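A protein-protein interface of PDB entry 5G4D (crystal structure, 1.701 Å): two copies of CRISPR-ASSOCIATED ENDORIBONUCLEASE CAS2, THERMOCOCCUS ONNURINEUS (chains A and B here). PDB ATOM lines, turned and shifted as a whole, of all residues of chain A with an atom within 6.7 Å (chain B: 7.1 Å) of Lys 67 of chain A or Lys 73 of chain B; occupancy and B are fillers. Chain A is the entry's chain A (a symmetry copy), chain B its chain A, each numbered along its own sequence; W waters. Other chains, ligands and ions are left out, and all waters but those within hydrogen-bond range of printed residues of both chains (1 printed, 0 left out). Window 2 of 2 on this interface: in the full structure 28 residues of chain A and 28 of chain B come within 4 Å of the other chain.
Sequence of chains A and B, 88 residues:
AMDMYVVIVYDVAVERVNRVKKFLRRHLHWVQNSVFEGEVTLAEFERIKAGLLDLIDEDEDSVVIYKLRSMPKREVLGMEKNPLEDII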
ATOM      1  N   MET A   4     -15.376  -4.868  -1.143  1.00  0.00           N
ATOM      2  CA  MET A   4     -16.183  -3.714  -0.764  1.00  0.00           C
ATOM      3  C   MET A   4     -17.096  -3.320  -1.918  1.00  0.00           C
ATOM      4  O   MET A   4     -17.086  -3.925  -2.992  1.00  0.00           O
ATOM      5  CB  MET A   4     -15.306  -2.543  -0.292  1.00  0.00           C
ATOM      6  CG  MET A   4     -14.179  -2.088  -1.187  1.00  0.00           C
ATOM      7  SD  MET A   4     -13.054  -0.998  -0.253  1.00  0.00           S
ATOM      8  CE  MET A   4     -11.972  -0.429  -1.569  1.00  0.00           C
ATOM      9  N   TYR A   5     -17.931  -2.316  -1.665  1.00  0.00           N
ATOM     10  CA  TYR A   5     -18.838  -1.758  -2.658  1.00  0.00           C
ATOM     11  C   TYR A   5     -18.504  -0.280  -2.816  1.00  0.00           C
ATOM     12  O   TYR A   5     -18.329   0.420  -1.820  1.00  0.00           O
ATOM     13  CB  TYR A   5     -20.299  -1.936  -2.215  1.00  0.00           C
ATOM     14  CG  TYR A   5     -21.298  -1.763  -3.321  1.00  0.00           C
ATOM     15  CD1 TYR A   5     -21.744  -0.495  -3.688  1.00  0.00           C
ATOM     16  CD2 TYR A   5     -21.813  -2.865  -4.000  1.00  0.00           C
ATOM     17  CE1 TYR A   5     -22.652  -0.329  -4.718  1.00  0.00           C
ATOM     18  CE2 TYR A   5     -22.725  -2.708  -5.026  1.00  0.00           C
ATOM     19  CZ  TYR A   5     -23.138  -1.437  -5.387  1.00  0.00           C
ATOM     20  OH  TYR A   5     -24.042  -1.259  -6.405  1.00  0.00           O
ATOM     21  N   VAL A   6     -18.397   0.197  -4.055  1.00  0.00           N
ATOM     22  CA  VAL A   6     -17.993   1.586  -4.267  1.00  0.00           C
ATOM     23  C   VAL A   6     -19.078   2.359  -5.004  1.00  0.00           C
ATOM     24  O   VAL A   6     -19.837   1.817  -5.815  1.00  0.00           O
ATOM     25  CB  VAL A   6     -16.651   1.700  -5.028  1.00  0.00           C
ATOM     26  CG1 VAL A   6     -15.506   1.161  -4.167  1.00  0.00           C
ATOM     27  CG2 VAL A   6     -16.730   0.982  -6.379  1.00  0.00           C
ATOM     28  N   VAL A   7     -19.154   3.650  -4.696  1.00  0.00           N
ATOM     29  CA  VAL A   7     -19.891   4.621  -5.504  1.00  0.00           C
ATOM     30  C   VAL A   7     -18.868   5.652  -5.928  1.00  0.00           C
ATOM     31  O   VAL A   7     -18.195   6.242  -5.073  1.00  0.00           O
ATOM     32  CB  VAL A   7     -21.044   5.298  -4.738  1.00  0.00           C
ATOM     33  CG1 VAL A   7     -21.690   6.381  -5.621  1.00  0.00           C
ATOM     34  CG2 VAL A   7     -22.070   4.282  -4.252  1.00  0.00           C
ATOM     35  N   PHE A  45     -10.235  -2.617  -7.005  1.00  0.00           N
ATOM     36  CA  PHE A  45     -10.260  -1.207  -6.626  1.00  0.00           C
ATOM     37  C   PHE A  45      -8.925  -0.531  -6.924  1.00  0.00           C
ATOM     38  O   PHE A  45      -8.894   0.600  -7.424  1.00  0.00           O
ATOM     39  CB  PHE A  45     -10.614  -1.024  -5.148  1.00  0.00           C
ATOM     40  CG  PHE A  45     -10.305   0.357  -4.653  1.00  0.00           C
ATOM     41  CD1 PHE A  45     -11.096   1.428  -5.035  1.00  0.00           C
ATOM     42  CD2 PHE A  45      -9.189   0.598  -3.875  1.00  0.00           C
ATOM     43  CE1 PHE A  45     -10.796   2.714  -4.617  1.00  0.00           C
ATOM     44  CE2 PHE A  45      -8.881   1.876  -3.456  1.00  0.00           C
ATOM     45  CZ  PHE A  45      -9.684   2.937  -3.831  1.00  0.00           C
ATOM     46  N   GLU A  46      -7.807  -1.210  -6.637  1.00  0.00           N
ATOM     47  CA  GLU A  46      -6.502  -0.617  -6.922  1.00  0.00           C
ATOM     48  C   GLU A  46      -6.322  -0.377  -8.413  1.00  0.00           C
ATOM     49  O   GLU A  46      -5.716   0.622  -8.817  1.00  0.00           O
ATOM     50  CB  GLU A  46      -5.373  -1.510  -6.395  1.00  0.00           C
ATOM     51  CG  GLU A  46      -5.289  -1.571  -4.886  1.00  0.00           C
ATOM     52  CD  GLU A  46      -5.058  -0.211  -4.251  1.00  0.00           C
ATOM     53  OE1 GLU A  46      -4.336   0.619  -4.840  1.00  0.00           O
ATOM     54  OE2 GLU A  46      -5.607   0.031  -3.156  1.00  0.00           O
ATOM     55  N   LYS A  49      -8.520   2.644  -9.409  1.00  0.00           N
ATOM     56  CA  LYS A  49      -7.840   3.866  -8.989  1.00  0.00           C
ATOM     57  C   LYS A  49      -6.666   4.186  -9.909  1.00  0.00           C
ATOM     58  O   LYS A  49      -6.494   5.333 -10.337  1.00  0.00           O
ATOM     59  CB  LYS A  49      -7.379   3.733  -7.538  1.00  0.00           C
ATOM     60  CG  LYS A  49      -6.484   4.865  -7.068  1.00  0.00           C
ATOM     61  CD  LYS A  49      -6.081   4.678  -5.620  1.00  0.00           C
ATOM     62  CE  LYS A  49      -4.969   5.644  -5.236  1.00  0.00           C
ATOM     63  NZ  LYS A  49      -4.559   5.452  -3.812  1.00  0.00           N
ATOM     64  N   ILE A  65     -14.367   8.505  -4.435  1.00  0.00           N
ATOM     65  CA  ILE A  65     -14.700   7.089  -4.358  1.00  0.00           C
ATOM     66  C   ILE A  65     -15.214   6.815  -2.949  1.00  0.00           C
ATOM     67  O   ILE A  65     -14.426   6.701  -1.995  1.00  0.00           O
ATOM     68  CB  ILE A  65     -13.495   6.201  -4.698  1.00  0.00           C
ATOM     69  CG1 ILE A  65     -12.931   6.603  -6.064  1.00  0.00           C
ATOM     70  CG2 ILE A  65     -13.897   4.730  -4.659  1.00  0.00           C
ATOM     71  CD1 ILE A  65     -11.649   5.866  -6.430  1.00  0.00           C
ATOM     72  N   TYR A  66     -16.535   6.673  -2.815  1.00  0.00           N
ATOM     73  CA  TYR A  66     -17.116   6.242  -1.546  1.00  0.00           C
ATOM     74  C   TYR A  66     -16.906   4.744  -1.393  1.00  0.00           C
ATOM     75  O   TYR A  66     -17.185   3.984  -2.324  1.00  0.00           O
ATOM     76  CB  TYR A  66     -18.609   6.568  -1.508  1.00  0.00           C
ATOM     77  CG  TYR A  66     -18.900   8.052  -1.553  1.00  0.00           C
ATOM     78  CD1 TYR A  66     -18.827   8.822  -0.402  1.00  0.00           C
ATOM     79  CD2 TYR A  66     -19.250   8.681  -2.751  1.00  0.00           C
ATOM     80  CE1 TYR A  66     -19.091  10.177  -0.433  1.00  0.00           C
ATOM     81  CE2 TYR A  66     -19.508  10.039  -2.798  1.00  0.00           C
ATOM     82  CZ  TYR A  66     -19.427  10.779  -1.628  1.00  0.00           C
ATOM     83  OH  TYR A  66     -19.683  12.129  -1.663  1.00  0.00           O
ATOM     84  N   LYS A  67     -16.414   4.312  -0.217  1.00  0.00           N
ATOM     85  CA  LYS A  67     -16.078   2.912   0.024  1.00  0.00           C
ATOM     86  C   LYS A  67     -17.034   2.376   1.082  1.00  0.00           C
ATOM     87  O   LYS A  67     -17.004   2.836   2.233  1.00  0.00           O
ATOM     88  CB  LYS A  67     -14.627   2.757   0.468  1.00  0.00           C
ATOM     89  CG  LYS A  67     -13.633   3.404  -0.474  1.00  0.00           C
ATOM     90  CD  LYS A  67     -12.251   3.494   0.144  1.00  0.00           C
ATOM     91  CE  LYS A  67     -11.213   3.471  -0.955  1.00  0.00           C
ATOM     92  NZ  LYS A  67      -9.817   3.900  -0.559  1.00  0.00           N
ATOM     93  N   LEU A  68     -17.880   1.422   0.674  1.00  0.00           N
ATOM     94  CA  LEU A  68     -18.991   0.941   1.488  1.00  0.00           C
ATOM     95  C   LEU A  68     -18.873  -0.559   1.719  1.00  0.00           C
ATOM     96  O   LEU A  68     -18.159  -1.261   1.003  1.00  0.00           O
ATOM     97  CB  LEU A  68     -20.338   1.269   0.836  1.00  0.00           C
ATOM     98  CG  LEU A  68     -20.469   2.719   0.358  1.00  0.00           C
ATOM     99  CD1 LEU A  68     -21.716   2.900  -0.482  1.00  0.00           C
ATOM    100  CD2 LEU A  68     -20.475   3.667   1.548  1.00  0.00           C
ATOM    101  N   ARG A  69     -19.583  -1.046   2.737  1.00  0.00           N
ATOM    102  CA  ARG A  69     -19.457  -2.443   3.142  1.00  0.00           C
ATOM    103  C   ARG A  69     -20.261  -3.371   2.248  1.00  0.00           C
ATOM    104  O   ARG A  69     -19.905  -4.548   2.091  1.00  0.00           O
ATOM    105  CB  ARG A  69     -19.905  -2.589   4.596  1.00  0.00           C
ATOM    106  CG  ARG A  69     -18.994  -1.849   5.539  1.00  0.00           C
ATOM    107  CD  ARG A  69     -19.633  -1.650   6.916  1.00  0.00           C
ATOM    108  NE  ARG A  69     -18.730  -0.920   7.787  1.00  0.00           N
ATOM    109  CZ  ARG A  69     -17.647  -1.474   8.327  1.00  0.00           C
ATOM    110  NH1 ARG A  69     -17.365  -2.735   8.061  1.00  0.00           N
ATOM    111  NH2 ARG A  69     -16.831  -0.777   9.110  1.00  0.00           N
ATOM    112  N   SER B  70     -24.001   6.270   8.556  1.00  0.00           N
ATOM    113  CA  SER B  70     -23.094   7.290   9.055  1.00  0.00           C
ATOM    114  C   SER B  70     -22.295   7.796   7.868  1.00  0.00           C
ATOM    115  O   SER B  70     -22.393   7.257   6.759  1.00  0.00           O
ATOM    116  CB  SER B  70     -22.166   6.731  10.136  1.00  0.00           C
ATOM    117  OG  SER B  70     -21.366   5.694   9.590  1.00  0.00           O
ATOM    118  N   MET B  71     -21.471   8.807   8.113  1.00  0.00           N
ATOM    119  CA  MET B  71     -20.651   9.366   7.054  1.00  0.00           C
ATOM    120  C   MET B  71     -19.737   8.285   6.484  1.00  0.00           C
ATOM    121  O   MET B  71     -19.025   7.609   7.249  1.00  0.00           O
ATOM    122  CB  MET B  71     -19.831  10.543   7.571  1.00  0.00           C
ATOM    123  CG  MET B  71     -19.001  11.226   6.507  1.00  0.00           C
ATOM    124  SD  MET B  71     -18.009  12.560   7.206  1.00  0.00           S
ATOM    125  CE  MET B  71     -19.007  14.008   6.955  1.00  0.00           C
ATOM    126  N   PRO B  72     -19.770   8.049   5.179  1.00  0.00           N
ATOM    127  CA  PRO B  72     -18.971   6.979   4.591  1.00  0.00           C
ATOM    128  C   PRO B  72     -17.516   7.377   4.427  1.00  0.00           C
ATOM    129  O   PRO B  72     -17.172   8.550   4.253  1.00  0.00           O
ATOM    130  CB  PRO B  72     -19.636   6.758   3.226  1.00  0.00           C
ATOM    131  CG  PRO B  72     -20.215   8.109   2.876  1.00  0.00           C
ATOM    132  CD  PRO B  72     -20.667   8.694   4.199  1.00  0.00           C
ATOM    133  N   LYS B  73     -16.648   6.371   4.478  1.00  0.00           N
ATOM    134  CA  LYS B  73     -15.267   6.613   4.119  1.00  0.00           C
ATOM    135  C   LYS B  73     -15.176   6.879   2.615  1.00  0.00           C
ATOM    136  O   LYS B  73     -15.993   6.398   1.825  1.00  0.00           O
ATOM    137  CB  LYS B  73     -14.382   5.431   4.515  1.00  0.00           C
ATOM    138  CG  LYS B  73     -12.940   5.658   4.140  1.00  0.00           C
ATOM    139  CD  LYS B  73     -12.019   4.653   4.752  1.00  0.00           C
ATOM    140  CE  LYS B  73     -12.553   3.308   4.438  1.00  0.00           C
ATOM    141  NZ  LYS B  73     -11.893   2.766   3.230  1.00  0.00           N
ATOM    142  N   ARG B  74     -14.207   7.697   2.226  1.00  0.00           N
ATOM    143  CA  ARG B  74     -14.027   7.973   0.807  1.00  0.00           C
ATOM    144  C   ARG B  74     -12.572   8.295   0.530  1.00  0.00           C
ATOM    145  O   ARG B  74     -11.835   8.739   1.413  1.00  0.00           O
ATOM    146  CB  ARG B  74     -14.938   9.117   0.335  1.00  0.00           C
ATOM    147  CG  ARG B  74     -14.401  10.539   0.546  1.00  0.00           C
ATOM    148  CD  ARG B  74     -14.526  11.008   2.000  1.00  0.00           C
ATOM    149  NE  ARG B  74     -15.829  10.705   2.601  1.00  0.00           N
ATOM    150  CZ  ARG B  74     -16.926  11.438   2.419  1.00  0.00           C
ATOM    151  NH1 ARG B  74     -16.895  12.516   1.634  1.00  0.00           N
ATOM    152  NH2 ARG B  74     -18.057  11.074   2.996  1.00  0.00           N
ATOM    153  N   GLU B  75     -12.168   8.054  -0.718  1.00  0.00           N
ATOM    154  CA  GLU B  75     -10.863   8.456  -1.227  1.00  0.00           C
ATOM    155  C   GLU B  75     -11.076   9.446  -2.360  1.00  0.00           C
ATOM    156  O   GLU B  75     -11.946   9.242  -3.206  1.00  0.00           O
ATOM    157  CB  GLU B  75     -10.062   7.256  -1.730  1.00  0.00           C
ATOM    158  CG  GLU B  75      -8.804   7.657  -2.481  1.00  0.00           C
ATOM    159  CD  GLU B  75      -7.750   6.571  -2.519  1.00  0.00           C
ATOM    160  OE1 GLU B  75      -8.070   5.394  -2.221  1.00  0.00           O
ATOM    161  OE2 GLU B  75      -6.586   6.908  -2.840  1.00  0.00           O
ATOM    162  N   VAL B  76     -10.291  10.519  -2.370  1.00  0.00           N
ATOM    163  CA  VAL B  76     -10.378  11.547  -3.398  1.00  0.00           C
ATOM    164  C   VAL B  76      -9.160  11.425  -4.299  1.00  0.00           C
ATOM    165  O   VAL B  76      -8.025  11.353  -3.811  1.00  0.00           O
ATOM    166  CB  VAL B  76     -10.469  12.955  -2.788  1.00  0.00           C
ATOM    167  CG1 VAL B  76     -10.583  14.005  -3.887  1.00  0.00           C
ATOM    168  CG2 VAL B  76     -11.648  13.041  -1.839  1.00  0.00           C
HETATM  169  O   HOH W   1     -17.601   3.598   4.760  1.00  0.00           O
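O of Val 7 of chain A is in hydrogen-bond range of N of Tyr 66 of chain A (2.8 Å). The backbone NH of Leu 68 of chain A is in hydrogen-bond range of the backbone carbonyl oxygen of Tyr 5 of chain A (2.7 Å). The backbone carbonyl oxygen (O) of Pro 72 of chain B is in hydrogen-bond range of the guanidinium group (NH2) of Arg 74 of chain B.
Among the printed residues, merely in contact across the chains: Ile 65 of chain A with Arg 74 of chain B, Phe 45 of chain A with Glu 75 of chain B, Tyr 66 of chain A with Lys 73 of chain B, Leu 68 of chain A with Pro 72 of chain B, Tyr 66 of chain A with Pro 72 of chain B and Tyr 66 of chain A with Arg 74 of chain B.
NZ of Lys 67 of chain A is in salt-bridge range of OE1 of Glu 75 of chain B (2.8 Å). N of Lys 67 of chain A lies within hydrogen-bond range of O of Lys 73 of chain B. The backbone carbonyl oxygen (O) of Glu 75 of chain B is in hydrogen-bond range of the backbone NH (N) of Ile 65 of chain A (2.8 Å). The side-chain carboxylate of Glu 75 of chain B lies within salt-bridge range of the side-chain amino group of Lys 49 of chain A (2.7 Å).
Of the 7 printed residues of chain B, 4 touch a printed residue of chain A. Of the 12 printed residues of chain A, 6 touch a printed residue of chain B. Hydrophobic or aromatic side chains of chain A within 4 Å of the printed part of chain B: Phe 45, Ile 65, Tyr 66 and Leu 68. Among the printed residues, 10 pairs touch across the chains.
No position is printed for both chains. Of the 10 pairs that touch across the chains among the printed residues, none has its exchanged pair printed and touching as well.
Of the printed residues of chain A, Lys 73 of chain B touches Tyr 66 (3.6 Å) and Lys 67 (2.9 Å). Of the printed residues of chain A, Pro 72 of chain B touches Tyr 66 (3.6 Å) and Leu 68 (3.6 Å). Printed residues of chain B within 4 Å of Tyr 66 of chain A: Pro 72 (3.6 Å), Lys 73 (3.6 Å) and Arg 74 (3.7 Å). Of the printed residues of chain B, Ile 65 of chain A touches Arg 74 and Glu 75. Of the printed residues of chain A, Arg 74 of chain B touches Ile 65 (3.1 Å) and Tyr 66 (3.7 Å). Arg 69 of chain A touches none of the printed residues of chain B. Glu 46 of chain A touches none of the printed residues of chain B. The nearest printed residue of chain B that does not touch Lys 49 of chain A is Val 76 of chain B (6.6 Å).
Water W1 lies within hydrogen-bond range of O of Lys 67 of chain A (2.7 Å) and N of Lys 73 of chain B (2.9 Å).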
